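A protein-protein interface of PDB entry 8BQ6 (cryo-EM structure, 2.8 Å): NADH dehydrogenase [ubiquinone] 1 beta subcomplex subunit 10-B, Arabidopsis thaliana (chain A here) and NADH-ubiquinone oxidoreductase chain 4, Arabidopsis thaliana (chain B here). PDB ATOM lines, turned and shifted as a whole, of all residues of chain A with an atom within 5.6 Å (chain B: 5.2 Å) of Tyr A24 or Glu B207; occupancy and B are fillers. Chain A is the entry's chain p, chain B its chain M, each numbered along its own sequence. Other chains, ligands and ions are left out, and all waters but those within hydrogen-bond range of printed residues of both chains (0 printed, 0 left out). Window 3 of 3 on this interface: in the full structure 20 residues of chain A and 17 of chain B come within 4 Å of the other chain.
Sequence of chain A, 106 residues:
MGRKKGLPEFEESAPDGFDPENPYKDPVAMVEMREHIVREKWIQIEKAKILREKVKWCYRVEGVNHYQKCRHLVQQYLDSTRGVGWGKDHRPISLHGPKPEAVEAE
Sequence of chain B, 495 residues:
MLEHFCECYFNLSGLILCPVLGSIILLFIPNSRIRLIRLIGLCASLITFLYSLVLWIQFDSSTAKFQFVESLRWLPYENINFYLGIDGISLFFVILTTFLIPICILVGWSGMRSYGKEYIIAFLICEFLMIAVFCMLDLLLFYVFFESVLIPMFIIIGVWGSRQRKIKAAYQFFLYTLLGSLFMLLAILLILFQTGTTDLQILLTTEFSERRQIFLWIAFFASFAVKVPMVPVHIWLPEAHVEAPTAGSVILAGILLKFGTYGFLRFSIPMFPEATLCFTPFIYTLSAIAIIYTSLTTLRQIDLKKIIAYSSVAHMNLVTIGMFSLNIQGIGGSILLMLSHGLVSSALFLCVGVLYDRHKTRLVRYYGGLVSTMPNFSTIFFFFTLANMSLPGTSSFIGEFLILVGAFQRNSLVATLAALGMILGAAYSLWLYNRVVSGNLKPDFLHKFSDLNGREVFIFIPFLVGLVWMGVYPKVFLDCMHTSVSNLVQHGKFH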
ATOM      1  N   ASP A  19      32.290 -22.300 -11.121  1.00  0.00           N
ATOM      2  CA  ASP A  19      33.369 -21.374 -11.542  1.00  0.00           C
ATOM      3  C   ASP A  19      33.958 -20.789 -10.258  1.00  0.00           C
ATOM      4  O   ASP A  19      33.241 -20.058  -9.566  1.00  0.00           O
ATOM      5  CB  ASP A  19      32.865 -20.322 -12.534  1.00  0.00           C
ATOM      6  CG  ASP A  19      33.982 -19.655 -13.322  1.00  0.00           C
ATOM      7  OD1 ASP A  19      35.103 -20.211 -13.348  1.00  0.00           O
ATOM      8  OD2 ASP A  19      33.726 -18.592 -13.915  1.00  0.00           O
ATOM      9  N   ASN A  22      33.834 -16.828 -10.169  1.00  0.00           N
ATOM     10  CA  ASN A  22      32.596 -16.153  -9.696  1.00  0.00           C
ATOM     11  C   ASN A  22      31.702 -17.206  -9.024  1.00  0.00           C
ATOM     12  O   ASN A  22      30.738 -17.673  -9.661  1.00  0.00           O
ATOM     13  CB  ASN A  22      31.896 -15.385 -10.824  1.00  0.00           C
ATOM     14  CG  ASN A  22      31.385 -16.259 -11.948  1.00  0.00           C
ATOM     15  OD1 ASN A  22      30.962 -17.388 -11.720  1.00  0.00           O
ATOM     16  ND2 ASN A  22      31.396 -15.735 -13.161  1.00  0.00           N
ATOM     17  N   PRO A  23      31.990 -17.613  -7.770  1.00  0.00           N
ATOM     18  CA  PRO A  23      31.223 -18.672  -7.098  1.00  0.00           C
ATOM     19  C   PRO A  23      29.710 -18.455  -7.005  1.00  0.00           C
ATOM     20  O   PRO A  23      29.022 -19.433  -6.809  1.00  0.00           O
ATOM     21  CB  PRO A  23      31.755 -18.564  -5.669  1.00  0.00           C
ATOM     22  CG  PRO A  23      33.181 -18.126  -5.845  1.00  0.00           C
ATOM     23  CD  PRO A  23      33.071 -17.084  -6.933  1.00  0.00           C
ATOM     24  N   TYR A  24      29.234 -17.218  -7.168  1.00  0.00           N
ATOM     25  CA  TYR A  24      27.827 -16.894  -6.983  1.00  0.00           C
ATOM     26  C   TYR A  24      27.075 -16.810  -8.311  1.00  0.00           C
ATOM     27  O   TYR A  24      26.133 -16.029  -8.475  1.00  0.00           O
ATOM     28  CB  TYR A  24      27.737 -15.584  -6.214  1.00  0.00           C
ATOM     29  CG  TYR A  24      27.916 -15.739  -4.723  1.00  0.00           C
ATOM     30  CD1 TYR A  24      26.854 -16.123  -3.929  1.00  0.00           C
ATOM     31  CD2 TYR A  24      29.150 -15.545  -4.114  1.00  0.00           C
ATOM     32  CE1 TYR A  24      26.993 -16.294  -2.584  1.00  0.00           C
ATOM     33  CE2 TYR A  24      29.305 -15.711  -2.746  1.00  0.00           C
ATOM     34  CZ  TYR A  24      28.207 -16.090  -1.991  1.00  0.00           C
ATOM     35  OH  TYR A  24      28.291 -16.270  -0.635  1.00  0.00           O
ATOM     36  N   LYS A  25      27.489 -17.620  -9.287  1.00  0.00           N
ATOM     37  CA  LYS A  25      26.835 -17.657 -10.592  1.00  0.00           C
ATOM     38  C   LYS A  25      26.045 -18.927 -10.825  1.00  0.00           C
ATOM     39  O   LYS A  25      24.970 -18.873 -11.420  1.00  0.00           O
ATOM     40  CB  LYS A  25      27.846 -17.527 -11.708  1.00  0.00           C
ATOM     41  CG  LYS A  25      27.280 -17.425 -13.103  1.00  0.00           C
ATOM     42  CD  LYS A  25      26.742 -16.019 -13.373  1.00  0.00           C
ATOM     43  CE  LYS A  25      26.201 -15.902 -14.787  1.00  0.00           C
ATOM     44  NZ  LYS A  25      27.150 -16.463 -15.782  1.00  0.00           N
ATOM     45  N   ASP A  26      26.554 -20.070 -10.381  1.00  0.00           N
ATOM     46  CA  ASP A  26      25.751 -21.285 -10.381  1.00  0.00           C
ATOM     47  C   ASP A  26      25.482 -21.655  -8.934  1.00  0.00           C
ATOM     48  O   ASP A  26      26.347 -22.250  -8.272  1.00  0.00           O
ATOM     49  CB  ASP A  26      26.456 -22.429 -11.113  1.00  0.00           C
ATOM     50  CG  ASP A  26      25.483 -23.479 -11.611  1.00  0.00           C
ATOM     51  OD1 ASP A  26      24.583 -23.864 -10.837  1.00  0.00           O
ATOM     52  OD2 ASP A  26      25.618 -23.919 -12.771  1.00  0.00           O
ATOM     53  N   PRO A  27      24.312 -21.315  -8.391  1.00  0.00           N
ATOM     54  CA  PRO A  27      24.093 -21.517  -6.950  1.00  0.00           C
ATOM     55  C   PRO A  27      23.943 -22.972  -6.569  1.00  0.00           C
ATOM     56  O   PRO A  27      24.448 -23.391  -5.520  1.00  0.00           O
ATOM     57  CB  PRO A  27      22.808 -20.720  -6.680  1.00  0.00           C
ATOM     58  CG  PRO A  27      22.635 -19.832  -7.880  1.00  0.00           C
ATOM     59  CD  PRO A  27      23.191 -20.604  -9.022  1.00  0.00           C
ATOM     60  N   MET A  30      27.175 -24.021  -6.366  1.00  0.00           N
ATOM     61  CA  MET A  30      27.797 -23.377  -5.214  1.00  0.00           C
ATOM     62  C   MET A  30      27.519 -24.153  -3.936  1.00  0.00           C
ATOM     63  O   MET A  30      28.431 -24.419  -3.144  1.00  0.00           O
ATOM     64  CB  MET A  30      27.268 -21.963  -5.067  1.00  0.00           C
ATOM     65  CG  MET A  30      27.615 -21.340  -3.749  1.00  0.00           C
ATOM     66  SD  MET A  30      26.225 -20.310  -3.293  1.00  0.00           S
ATOM     67  CE  MET A  30      26.282 -19.136  -4.624  1.00  0.00           C
ATOM     68  N   GLN B 194      16.270  -5.988  -2.140  1.00  0.00           N
ATOM     69  CA  GLN B 194      17.282  -6.591  -3.000  1.00  0.00           C
ATOM     70  C   GLN B 194      16.787  -7.843  -3.699  1.00  0.00           C
ATOM     71  O   GLN B 194      16.746  -7.915  -4.930  1.00  0.00           O
ATOM     72  CB  GLN B 194      18.529  -6.997  -2.219  1.00  0.00           C
ATOM     73  CG  GLN B 194      19.520  -5.942  -1.851  1.00  0.00           C
ATOM     74  CD  GLN B 194      20.912  -6.551  -1.864  1.00  0.00           C
ATOM     75  OE1 GLN B 194      21.593  -6.611  -0.846  1.00  0.00           O
ATOM     76  NE2 GLN B 194      21.316  -7.057  -3.022  1.00  0.00           N
ATOM     77  N   LEU B 204      20.761 -17.945   1.424  1.00  0.00           N
ATOM     78  CA  LEU B 204      22.071 -18.605   1.668  1.00  0.00           C
ATOM     79  C   LEU B 204      22.857 -18.767   0.359  1.00  0.00           C
ATOM     80  O   LEU B 204      24.050 -19.083   0.422  1.00  0.00           O
ATOM     81  CB  LEU B 204      21.786 -19.959   2.321  1.00  0.00           C
ATOM     82  CG  LEU B 204      21.164 -19.880   3.714  1.00  0.00           C
ATOM     83  CD1 LEU B 204      20.931 -21.265   4.294  1.00  0.00           C
ATOM     84  CD2 LEU B 204      22.013 -19.035   4.650  1.00  0.00           C
ATOM     85  N   THR B 205      22.214 -18.580  -0.790  1.00  0.00           N
ATOM     86  CA  THR B 205      22.863 -18.708  -2.087  1.00  0.00           C
ATOM     87  C   THR B 205      23.001 -17.379  -2.821  1.00  0.00           C
ATOM     88  O   THR B 205      23.374 -17.374  -4.001  1.00  0.00           O
ATOM     89  CB  THR B 205      22.089 -19.699  -2.954  1.00  0.00           C
ATOM     90  OG1 THR B 205      20.823 -19.125  -3.298  1.00  0.00           O
ATOM     91  CG2 THR B 205      21.862 -20.997  -2.209  1.00  0.00           C
ATOM     92  N   THR B 206      22.718 -16.259  -2.166  1.00  0.00           N
ATOM     93  CA  THR B 206      22.808 -14.949  -2.792  1.00  0.00           C
ATOM     94  C   THR B 206      23.975 -14.165  -2.205  1.00  0.00           C
ATOM     95  O   THR B 206      24.312 -14.293  -1.025  1.00  0.00           O
ATOM     96  CB  THR B 206      21.500 -14.170  -2.614  1.00  0.00           C
ATOM     97  OG1 THR B 206      20.392 -15.037  -2.876  1.00  0.00           O
ATOM     98  CG2 THR B 206      21.434 -13.010  -3.590  1.00  0.00           C
ATOM     99  N   GLU B 207      24.598 -13.350  -3.051  1.00  0.00           N
ATOM    100  CA  GLU B 207      25.780 -12.580  -2.688  1.00  0.00           C
ATOM    101  C   GLU B 207      25.358 -11.180  -2.257  1.00  0.00           C
ATOM    102  O   GLU B 207      24.511 -10.552  -2.905  1.00  0.00           O
ATOM    103  CB  GLU B 207      26.773 -12.528  -3.853  1.00  0.00           C
ATOM    104  CG  GLU B 207      26.275 -11.832  -5.111  1.00  0.00           C
ATOM    105  CD  GLU B 207      27.266 -11.929  -6.253  1.00  0.00           C
ATOM    106  OE1 GLU B 207      28.451 -12.223  -5.988  1.00  0.00           O
ATOM    107  OE2 GLU B 207      26.861 -11.700  -7.410  1.00  0.00           O
ATOM    108  N   PHE B 208      25.923 -10.713  -1.148  1.00  0.00           N
ATOM    109  CA  PHE B 208      25.697  -9.368  -0.639  1.00  0.00           C
ATOM    110  C   PHE B 208      26.982  -8.557  -0.751  1.00  0.00           C
ATOM    111  O   PHE B 208      28.083  -9.112  -0.722  1.00  0.00           O
ATOM    112  CB  PHE B 208      25.233  -9.402   0.820  1.00  0.00           C
ATOM    113  CG  PHE B 208      23.825  -9.896   1.011  1.00  0.00           C
ATOM    114  CD1 PHE B 208      22.746  -9.065   0.760  1.00  0.00           C
ATOM    115  CD2 PHE B 208      23.579 -11.192   1.440  1.00  0.00           C
ATOM    116  CE1 PHE B 208      21.448  -9.510   0.940  1.00  0.00           C
ATOM    117  CE2 PHE B 208      22.283 -11.646   1.615  1.00  0.00           C
ATOM    118  CZ  PHE B 208      21.216 -10.803   1.366  1.00  0.00           C
ATOM    119  N   SER B 209      26.837  -7.243  -0.894  1.00  0.00           N
ATOM    120  CA  SER B 209      28.001  -6.369  -0.898  1.00  0.00           C
ATOM    121  C   SER B 209      28.512  -6.173   0.524  1.00  0.00           C
ATOM    122  O   SER B 209      27.748  -6.226   1.490  1.00  0.00           O
ATOM    123  CB  SER B 209      27.656  -5.017  -1.516  1.00  0.00           C
ATOM    124  OG  SER B 209      26.692  -4.342  -0.730  1.00  0.00           O
ATOM    125  N   GLY B 492      30.290 -19.457   2.724  1.00  0.00           N
ATOM    126  CA  GLY B 492      30.908 -18.242   2.249  1.00  0.00           C
ATOM    127  C   GLY B 492      32.361 -18.380   1.853  1.00  0.00           C
ATOM    128  O   GLY B 492      32.953 -17.397   1.397  1.00  0.00           O
ATOM    129  N   PHE B 494      35.375 -21.134  -0.120  1.00  0.00           N
ATOM    130  CA  PHE B 494      35.500 -22.227  -1.075  1.00  0.00           C
ATOM    131  C   PHE B 494      36.919 -22.761  -1.103  1.00  0.00           C
ATOM    132  O   PHE B 494      37.429 -23.189  -2.142  1.00  0.00           O
ATOM    133  CB  PHE B 494      35.046 -21.783  -2.458  1.00  0.00           C
ATOM    134  CG  PHE B 494      33.637 -21.299  -2.478  1.00  0.00           C
ATOM    135  CD1 PHE B 494      32.591 -22.199  -2.520  1.00  0.00           C
ATOM    136  CD2 PHE B 494      33.353 -19.950  -2.414  1.00  0.00           C
ATOM    137  CE1 PHE B 494      31.288 -21.761  -2.519  1.00  0.00           C
ATOM    138  CE2 PHE B 494      32.051 -19.512  -2.405  1.00  0.00           C
ATOM    139  CZ  PHE B 494      31.018 -20.417  -2.466  1.00  0.00           C
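Tyr A24 touches just these residues of chain B: Thr B205, Thr B206 and Glu B207.
Of chain A, only Tyr A24 (3.4 Å) comes within 4 Å of Glu B207.
Printed residues of chain A within 4 Å of Thr B206: Tyr A24 (3.7 Å).
Printed residues of chain A within 4 Å of Phe B494: Pro A23 (3.4 Å) and Met A30 (3.8 Å).
Of the printed residues of chain A, Thr B205 touches Tyr A24, Pro A27 and Met A30.
Of the printed residues of chain B, Pro A23 touches Phe B494 (3.4 Å).
Gly B492 touches none of the printed residues of chain A.
Phe B208 touches none of the printed residues of chain A.
The nearest residue of chain B that does not touch Tyr A24 is Gly B492 (4.4 Å).
The nearest printed residue of chain A that does not touch Glu B207 is Met A30 (6.2 Å).
Among the printed residues, pairs that only touch across the chains: Pro A23 with Phe B494 (3.4 Å), Tyr A24 with Thr B205 (3.7 Å), Tyr A24 with Thr B206 (3.7 Å), Tyr A24 with Glu B207 (3.4 Å), Pro A27 with Thr B205 (3.9 Å), Met A30 with Thr B205 (3.5 Å) and Met A30 with Phe B494 (3.8 Å).
Of the 8 printed residues of chain A, 4 touch a printed residue of chain B.
Hydrophobic or aromatic side chains of chain A that line the printed part of chain B: Pro A23, Tyr A24, Pro A27 and Met A30.
Printed residues of chain B that touch a printed residue of chain A: Thr B205, Thr B206, Glu B207 and Phe B494.
Along chain B the printed residues that touch a printed residue of chain A span positions 205 to 494.
Among the printed residues, 7 pairs touch across the chains.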
